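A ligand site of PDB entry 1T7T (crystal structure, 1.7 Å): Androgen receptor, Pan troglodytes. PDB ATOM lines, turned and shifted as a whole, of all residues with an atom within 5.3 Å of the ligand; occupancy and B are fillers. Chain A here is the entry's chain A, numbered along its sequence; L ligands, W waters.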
ATOM      1  N   LEU A  51      -9.180   6.680 -33.999  1.00  0.00           N
ATOM      2  CA  LEU A  51      -9.445   7.957 -33.349  1.00  0.00           C
ATOM      3  C   LEU A  51     -10.147   8.935 -34.299  1.00  0.00           C
ATOM      4  O   LEU A  51     -11.012   9.707 -33.862  1.00  0.00           O
ATOM      5  CB  LEU A  51      -8.164   8.566 -32.777  1.00  0.00           C
ATOM      6  CG  LEU A  51      -7.860   8.152 -31.326  1.00  0.00           C
ATOM      7  CD1 LEU A  51      -8.959   8.671 -30.398  1.00  0.00           C
ATOM      8  CD2 LEU A  51      -7.762   6.638 -31.231  1.00  0.00           C
ATOM      9  N   LEU A  54     -13.678   7.986 -34.066  1.00  0.00           N
ATOM     10  CA  LEU A  54     -14.280   8.365 -32.786  1.00  0.00           C
ATOM     11  C   LEU A  54     -14.591   9.862 -32.842  1.00  0.00           C
ATOM     12  O   LEU A  54     -15.639  10.294 -32.359  1.00  0.00           O
ATOM     13  CB  LEU A  54     -13.341   8.051 -31.614  1.00  0.00           C
ATOM     14  CG  LEU A  54     -13.319   6.591 -31.150  1.00  0.00           C
ATOM     15  CD1 LEU A  54     -12.134   6.353 -30.212  1.00  0.00           C
ATOM     16  CD2 LEU A  54     -14.620   6.261 -30.449  1.00  0.00           C
ATOM     17  N   ASN A  55     -13.694  10.647 -33.420  1.00  0.00           N
ATOM     18  CA  ASN A  55     -13.915  12.090 -33.530  1.00  0.00           C
ATOM     19  C   ASN A  55     -15.127  12.415 -34.400  1.00  0.00           C
ATOM     20  O   ASN A  55     -15.929  13.287 -34.066  1.00  0.00           O
ATOM     21  CB  ASN A  55     -12.683  12.801 -34.096  1.00  0.00           C
ATOM     22  CG  ASN A  55     -11.536  12.867 -33.107  1.00  0.00           C
ATOM     23  OD1 ASN A  55     -11.734  12.742 -31.896  1.00  0.00           O
ATOM     24  ND2 ASN A  55     -10.314  13.077 -33.603  1.00  0.00           N
ATOM     25  N   LEU A  57     -17.611  10.437 -34.921  1.00  0.00           N
ATOM     26  CA  LEU A  57     -18.783   9.981 -34.163  1.00  0.00           C
ATOM     27  C   LEU A  57     -19.159  11.069 -33.165  1.00  0.00           C
ATOM     28  O   LEU A  57     -20.345  11.359 -32.961  1.00  0.00           O
ATOM     29  CB  LEU A  57     -18.477   8.688 -33.414  1.00  0.00           C
ATOM     30  CG  LEU A  57     -19.637   8.160 -32.565  1.00  0.00           C
ATOM     31  CD1 LEU A  57     -20.846   7.883 -33.445  1.00  0.00           C
ATOM     32  CD2 LEU A  57     -19.197   6.883 -31.852  1.00  0.00           C
ATOM     33  N   GLY A  58     -18.159  11.683 -32.537  1.00  0.00           N
ATOM     34  CA  GLY A  58     -18.427  12.735 -31.590  1.00  0.00           C
ATOM     35  C   GLY A  58     -19.137  13.894 -32.279  1.00  0.00           C
ATOM     36  O   GLY A  58     -20.109  14.446 -31.752  1.00  0.00           O
ATOM     37  N   GLN A  61     -22.677  12.770 -32.990  1.00  0.00           N
ATOM     38  CA  GLN A  61     -23.461  12.703 -31.763  1.00  0.00           C
ATOM     39  C   GLN A  61     -23.784  14.088 -31.195  1.00  0.00           C
ATOM     40  O   GLN A  61     -24.863  14.294 -30.640  1.00  0.00           O
ATOM     41  CB  GLN A  61     -22.732  11.870 -30.694  1.00  0.00           C
ATOM     42  CG  GLN A  61     -22.670  10.378 -31.027  1.00  0.00           C
ATOM     43  CD  GLN A  61     -22.547   9.496 -29.808  1.00  0.00           C
ATOM     44  OE1 GLN A  61     -22.418   8.275 -29.925  1.00  0.00           O
ATOM     45  NE2 GLN A  61     -22.593  10.093 -28.629  1.00  0.00           N
ATOM     46  N   TRP A  91     -21.011  17.425 -22.671  1.00  0.00           N
ATOM     47  CA  TRP A  91     -21.111  16.416 -23.717  1.00  0.00           C
ATOM     48  C   TRP A  91     -20.316  15.125 -23.502  1.00  0.00           C
ATOM     49  O   TRP A  91     -20.825  14.039 -23.762  1.00  0.00           O
ATOM     50  CB  TRP A  91     -20.767  17.003 -25.091  1.00  0.00           C
ATOM     51  CG  TRP A  91     -19.378  17.506 -25.223  1.00  0.00           C
ATOM     52  CD1 TRP A  91     -18.907  18.718 -24.838  1.00  0.00           C
ATOM     53  CD2 TRP A  91     -18.254  16.783 -25.750  1.00  0.00           C
ATOM     54  NE1 TRP A  91     -17.560  18.805 -25.085  1.00  0.00           N
ATOM     55  CE2 TRP A  91     -17.134  17.626 -25.645  1.00  0.00           C
ATOM     56  CE3 TRP A  91     -18.091  15.503 -26.287  1.00  0.00           C
ATOM     57  CZ2 TRP A  91     -15.858  17.239 -26.063  1.00  0.00           C
ATOM     58  CZ3 TRP A  91     -16.824  15.113 -26.709  1.00  0.00           C
ATOM     59  CH2 TRP A  91     -15.724  15.980 -26.596  1.00  0.00           C
ATOM     60  N   MET A  92     -19.080  15.230 -23.015  1.00  0.00           N
ATOM     61  CA  MET A  92     -18.275  14.025 -22.793  1.00  0.00           C
ATOM     62  C   MET A  92     -18.966  13.051 -21.829  1.00  0.00           C
ATOM     63  O   MET A  92     -19.133  11.878 -22.143  1.00  0.00           O
ATOM     64  CB  MET A  92     -16.886  14.392 -22.265  1.00  0.00           C
ATOM     65  CG  MET A  92     -15.920  13.197 -22.195  1.00  0.00           C
ATOM     66  SD  MET A  92     -15.355  12.629 -23.837  1.00  0.00           S
ATOM     67  CE  MET A  92     -14.002  13.818 -24.144  1.00  0.00           C
ATOM     68  N   MET A  95     -22.193  11.557 -23.427  1.00  0.00           N
ATOM     69  CA  MET A  95     -21.906  10.564 -24.453  1.00  0.00           C
ATOM     70  C   MET A  95     -21.313   9.283 -23.892  1.00  0.00           C
ATOM     71  O   MET A  95     -21.632   8.191 -24.366  1.00  0.00           O
ATOM     72  CB  MET A  95     -20.991  11.146 -25.516  1.00  0.00           C
ATOM     73  CG  MET A  95     -21.635  12.269 -26.317  1.00  0.00           C
ATOM     74  SD  MET A  95     -20.570  12.846 -27.630  1.00  0.00           S
ATOM     75  CE  MET A  95     -21.540  14.227 -28.247  1.00  0.00           C
ATOM     76  N   VAL A  96     -20.464   9.400 -22.883  1.00  0.00           N
ATOM     77  CA  VAL A  96     -19.855   8.229 -22.264  1.00  0.00           C
ATOM     78  C   VAL A  96     -20.927   7.420 -21.546  1.00  0.00           C
ATOM     79  O   VAL A  96     -20.937   6.186 -21.613  1.00  0.00           O
ATOM     80  CB  VAL A  96     -18.751   8.639 -21.262  1.00  0.00           C
ATOM     81  CG1 VAL A  96     -18.362   7.445 -20.395  1.00  0.00           C
ATOM     82  CG2 VAL A  96     -17.530   9.161 -22.015  1.00  0.00           C
ATOM     83  N   MET A  99     -23.085   5.665 -24.093  1.00  0.00           N
ATOM     84  CA  MET A  99     -22.326   4.591 -24.715  1.00  0.00           C
ATOM     85  C   MET A  99     -22.252   3.394 -23.756  1.00  0.00           C
ATOM     86  O   MET A  99     -22.361   2.246 -24.170  1.00  0.00           O
ATOM     87  CB  MET A  99     -20.914   5.085 -25.084  1.00  0.00           C
ATOM     88  CG  MET A  99     -20.053   4.077 -25.854  1.00  0.00           C
ATOM     89  SD  MET A  99     -19.240   2.887 -24.783  1.00  0.00           S
ATOM     90  CE  MET A  99     -17.981   3.940 -24.014  1.00  0.00           C
ATOM     91  N   ARG A 102     -25.521   1.652 -24.018  1.00  0.00           N
ATOM     92  CA  ARG A 102     -25.619   0.942 -25.293  1.00  0.00           C
ATOM     93  C   ARG A 102     -24.823  -0.356 -25.212  1.00  0.00           C
ATOM     94  O   ARG A 102     -25.241  -1.393 -25.717  1.00  0.00           O
ATOM     95  CB  ARG A 102     -25.036   1.768 -26.446  1.00  0.00           C
ATOM     96  CG  ARG A 102     -25.898   2.900 -26.942  1.00  0.00           C
ATOM     97  CD  ARG A 102     -25.449   3.320 -28.339  1.00  0.00           C
ATOM     98  NE  ARG A 102     -24.117   3.925 -28.366  1.00  0.00           N
ATOM     99  CZ  ARG A 102     -23.836   5.167 -27.968  1.00  0.00           C
ATOM    100  NH1 ARG A 102     -24.804   5.953 -27.504  1.00  0.00           N
ATOM    101  NH2 ARG A 102     -22.602   5.625 -28.049  1.00  0.00           N
ATOM    102  N   PHE A 114     -19.531   1.918 -29.147  1.00  0.00           N
ATOM    103  CA  PHE A 114     -19.550   3.345 -29.463  1.00  0.00           C
ATOM    104  C   PHE A 114     -20.640   3.589 -30.502  1.00  0.00           C
ATOM    105  O   PHE A 114     -21.386   4.566 -30.413  1.00  0.00           O
ATOM    106  CB  PHE A 114     -18.178   3.781 -29.998  1.00  0.00           C
ATOM    107  CG  PHE A 114     -17.099   3.787 -28.944  1.00  0.00           C
ATOM    108  CD1 PHE A 114     -17.052   4.788 -27.977  1.00  0.00           C
ATOM    109  CD2 PHE A 114     -16.112   2.799 -28.938  1.00  0.00           C
ATOM    110  CE1 PHE A 114     -16.053   4.810 -27.007  1.00  0.00           C
ATOM    111  CE2 PHE A 114     -15.100   2.815 -27.968  1.00  0.00           C
ATOM    112  CZ  PHE A 114     -15.072   3.812 -27.008  1.00  0.00           C
ATOM    113  N   MET A 130      -5.885   4.434 -25.318  1.00  0.00           N
ATOM    114  CA  MET A 130      -6.613   4.897 -24.131  1.00  0.00           C
ATOM    115  C   MET A 130      -7.257   3.648 -23.521  1.00  0.00           C
ATOM    116  O   MET A 130      -8.437   3.611 -23.198  1.00  0.00           O
ATOM    117  CB  MET A 130      -7.653   5.983 -24.465  1.00  0.00           C
ATOM    118  CG  MET A 130      -8.536   5.675 -25.656  1.00  0.00           C
ATOM    119  SD  MET A 130      -9.737   7.009 -25.934  1.00  0.00           S
ATOM    120  CE  MET A 130     -11.178   6.327 -25.146  1.00  0.00           C
ATOM    121  N   MET A 137     -14.582   2.610 -18.717  1.00  0.00           N
ATOM    122  CA  MET A 137     -15.885   2.789 -19.339  1.00  0.00           C
ATOM    123  C   MET A 137     -16.609   1.436 -19.410  1.00  0.00           C
ATOM    124  O   MET A 137     -17.839   1.369 -19.347  1.00  0.00           O
ATOM    125  CB  MET A 137     -15.759   3.400 -20.735  1.00  0.00           C
ATOM    126  CG  MET A 137     -15.313   4.861 -20.723  1.00  0.00           C
ATOM    127  SD  MET A 137     -15.402   5.685 -22.338  1.00  0.00           S
ATOM    128  CE  MET A 137     -13.904   5.058 -23.124  1.00  0.00           C
ATOM    129  N   LEU A 223     -10.742  11.539 -20.310  1.00  0.00           N
ATOM    130  CA  LEU A 223     -10.949  11.635 -21.757  1.00  0.00           C
ATOM    131  C   LEU A 223     -10.751  13.078 -22.231  1.00  0.00           C
ATOM    132  O   LEU A 223     -10.279  13.310 -23.338  1.00  0.00           O
ATOM    133  CB  LEU A 223     -12.349  11.131 -22.131  1.00  0.00           C
ATOM    134  CG  LEU A 223     -12.558   9.628 -21.888  1.00  0.00           C
ATOM    135  CD1 LEU A 223     -14.023   9.272 -22.108  1.00  0.00           C
ATOM    136  CD2 LEU A 223     -11.658   8.818 -22.839  1.00  0.00           C
ATOM    137  N   PHE A 226      -7.071  13.403 -22.543  1.00  0.00           N
ATOM    138  CA  PHE A 226      -6.600  12.643 -23.691  1.00  0.00           C
ATOM    139  C   PHE A 226      -6.917  13.313 -25.018  1.00  0.00           C
ATOM    140  O   PHE A 226      -6.046  13.417 -25.888  1.00  0.00           O
ATOM    141  CB  PHE A 226      -7.206  11.237 -23.643  1.00  0.00           C
ATOM    142  CG  PHE A 226      -6.685  10.320 -24.715  1.00  0.00           C
ATOM    143  CD1 PHE A 226      -7.390  10.150 -25.906  1.00  0.00           C
ATOM    144  CD2 PHE A 226      -5.495   9.624 -24.538  1.00  0.00           C
ATOM    145  CE1 PHE A 226      -6.926   9.289 -26.900  1.00  0.00           C
ATOM    146  CE2 PHE A 226      -5.009   8.760 -25.528  1.00  0.00           C
ATOM    147  CZ  PHE A 226      -5.729   8.591 -26.712  1.00  0.00           C
ATOM    148  N   THR A 227      -8.147  13.784 -25.184  1.00  0.00           N
ATOM    149  CA  THR A 227      -8.520  14.401 -26.450  1.00  0.00           C
ATOM    150  C   THR A 227      -7.847  15.756 -26.630  1.00  0.00           C
ATOM    151  O   THR A 227      -7.499  16.152 -27.746  1.00  0.00           O
ATOM    152  CB  THR A 227     -10.055  14.539 -26.599  1.00  0.00           C
ATOM    153  OG1 THR A 227     -10.382  14.807 -27.964  1.00  0.00           O
ATOM    154  CG2 THR A 227     -10.593  15.670 -25.715  1.00  0.00           C
ATOM    155  N   LEU A 230      -4.422  15.036 -27.730  1.00  0.00           N
ATOM    156  CA  LEU A 230      -4.452  14.514 -29.089  1.00  0.00           C
ATOM    157  C   LEU A 230      -4.668  15.617 -30.131  1.00  0.00           C
ATOM    158  O   LEU A 230      -4.065  15.600 -31.195  1.00  0.00           O
ATOM    159  CB  LEU A 230      -5.536  13.440 -29.226  1.00  0.00           C
ATOM    160  CG  LEU A 230      -5.674  12.764 -30.586  1.00  0.00           C
ATOM    161  CD1 LEU A 230      -4.370  12.081 -30.981  1.00  0.00           C
ATOM    162  CD2 LEU A 230      -6.803  11.752 -30.519  1.00  0.00           C
ATOM    163  N   PHE A 241      -9.794  15.960 -36.790  1.00  0.00           N
ATOM    164  CA  PHE A 241     -10.778  16.488 -35.850  1.00  0.00           C
ATOM    165  C   PHE A 241     -11.762  17.353 -36.646  1.00  0.00           C
ATOM    166  O   PHE A 241     -11.347  18.315 -37.287  1.00  0.00           O
ATOM    167  CB  PHE A 241     -10.136  17.367 -34.779  1.00  0.00           C
ATOM    168  CG  PHE A 241      -9.553  16.604 -33.614  1.00  0.00           C
ATOM    169  CD1 PHE A 241      -8.302  16.009 -33.719  1.00  0.00           C
ATOM    170  CD2 PHE A 241     -10.257  16.489 -32.417  1.00  0.00           C
ATOM    171  CE1 PHE A 241      -7.763  15.303 -32.640  1.00  0.00           C
ATOM    172  CE2 PHE A 241      -9.722  15.792 -31.334  1.00  0.00           C
ATOM    173  CZ  PHE A 241      -8.465  15.194 -31.451  1.00  0.00           C
ATOM    174  N   MET A 245     -15.872  19.630 -33.038  1.00  0.00           N
ATOM    175  CA  MET A 245     -15.039  18.963 -32.046  1.00  0.00           C
ATOM    176  C   MET A 245     -13.780  19.795 -31.790  1.00  0.00           C
ATOM    177  O   MET A 245     -13.389  20.002 -30.639  1.00  0.00           O
ATOM    178  CB  MET A 245     -14.660  17.559 -32.526  1.00  0.00           C
ATOM    179  CG  MET A 245     -15.805  16.547 -32.474  1.00  0.00           C
ATOM    180  SD  MET A 245     -16.290  16.093 -30.786  1.00  0.00           S
ATOM    181  CE  MET A 245     -15.109  14.829 -30.447  1.00  0.00           C
ATOM    182  N   ILE A 249     -13.047  21.447 -28.107  1.00  0.00           N
ATOM    183  CA  ILE A 249     -11.894  20.913 -27.401  1.00  0.00           C
ATOM    184  C   ILE A 249     -10.797  21.946 -27.190  1.00  0.00           C
ATOM    185  O   ILE A 249      -9.983  21.819 -26.277  1.00  0.00           O
ATOM    186  CB  ILE A 249     -11.345  19.655 -28.131  1.00  0.00           C
ATOM    187  CG1 ILE A 249     -12.404  18.544 -28.043  1.00  0.00           C
ATOM    188  CG2 ILE A 249     -10.047  19.176 -27.485  1.00  0.00           C
ATOM    189  CD1 ILE A 249     -12.149  17.353 -28.932  1.00  0.00           C
HETATM  190  C1  LIG L   1     -17.889   9.525 -29.024  1.00  0.00           C
HETATM  191  C2  LIG L   1     -19.352   9.216 -28.665  1.00  0.00           C
HETATM  192  C3  LIG L   1     -19.321   8.010 -27.676  1.00  0.00           C
HETATM  193  O1  LIG L   1     -20.010   7.039 -27.918  1.00  0.00           O
HETATM  194  C4  LIG L   1     -18.407   8.109 -26.493  1.00  0.00           C
HETATM  195  C5  LIG L   1     -16.947   8.383 -26.932  1.00  0.00           C
HETATM  196  C6  LIG L   1     -15.957   8.491 -25.723  1.00  0.00           C
HETATM  197  C7  LIG L   1     -14.523   8.730 -26.239  1.00  0.00           C
HETATM  198  C8  LIG L   1     -14.416  10.034 -27.107  1.00  0.00           C
HETATM  199  C9  LIG L   1     -15.429   9.945 -28.300  1.00  0.00           C
HETATM  200  C10 LIG L   1     -16.913   9.716 -27.828  1.00  0.00           C
HETATM  201  C11 LIG L   1     -15.284  11.230 -29.169  1.00  0.00           C
HETATM  202  C12 LIG L   1     -13.873  11.552 -29.678  1.00  0.00           C
HETATM  203  C13 LIG L   1     -12.822  11.530 -28.541  1.00  0.00           C
HETATM  204  C14 LIG L   1     -12.996  10.233 -27.674  1.00  0.00           C
HETATM  205  C15 LIG L   1     -11.830  10.355 -26.683  1.00  0.00           C
HETATM  206  C16 LIG L   1     -10.671  10.803 -27.616  1.00  0.00           C
HETATM  207  C17 LIG L   1     -11.362  11.305 -28.906  1.00  0.00           C
HETATM  208  O2  LIG L   1     -10.696  12.498 -29.377  1.00  0.00           O
HETATM  209  C18 LIG L   1     -12.988  12.838 -27.665  1.00  0.00           C
HETATM  210  C19 LIG L   1     -17.384  10.967 -26.962  1.00  0.00           C
HETATM  211  O   HOH W   1     -22.942   8.292 -26.735  1.00  0.00           O
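NE2 of Gln 61 sits close to SD of Met 95 (3.6 Å). The guanidinium group of Arg 102 lies within hydrogen-bond range of the backbone carbonyl oxygen of Phe 114 (2.9 Å). ND2 of Asn 55 lies close to O of Leu 51, 3.5 Å away. NH2 of Arg 102 is in hydrogen-bond range of OE1 of Gln 61, 3.3 Å away.
Merely in contact with the ligand: Leu 51 (3.9 Å), Leu 54 (3.3 Å), Leu 57 (3.95 Å), Met 92 (3.8 Å), Met 95 (3.8 Å), Met 99 (3.6 Å), Phe 114 (3.7 Å), Phe 226 (3.8 Å), Phe 241 (3.95 Å) and Met 245 (3.6 Å).
Water W1 lies within hydrogen-bond range of NE2 of Gln 61 (2.6 Å), O of Met 95 (2.7 Å), NH2 of Arg 102 (3.0 Å) and O1 of the ligand (3.4 Å).
OE1 of Gln 61 lies close to O1 of the ligand (3.4 Å). NH2 of Arg 102 lies within hydrogen-bond range of O1 of the ligand. An oxygen (O2) of the ligand lies within hydrogen-bond range of the side-chain hydroxyl (OG1) of Thr 227, 2.7 Å away. The side-chain amide oxygen (OD1) of Asn 55 sits at hydrogen-bond distance from an oxygen (O2) of the ligand, 2.7 Å away.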
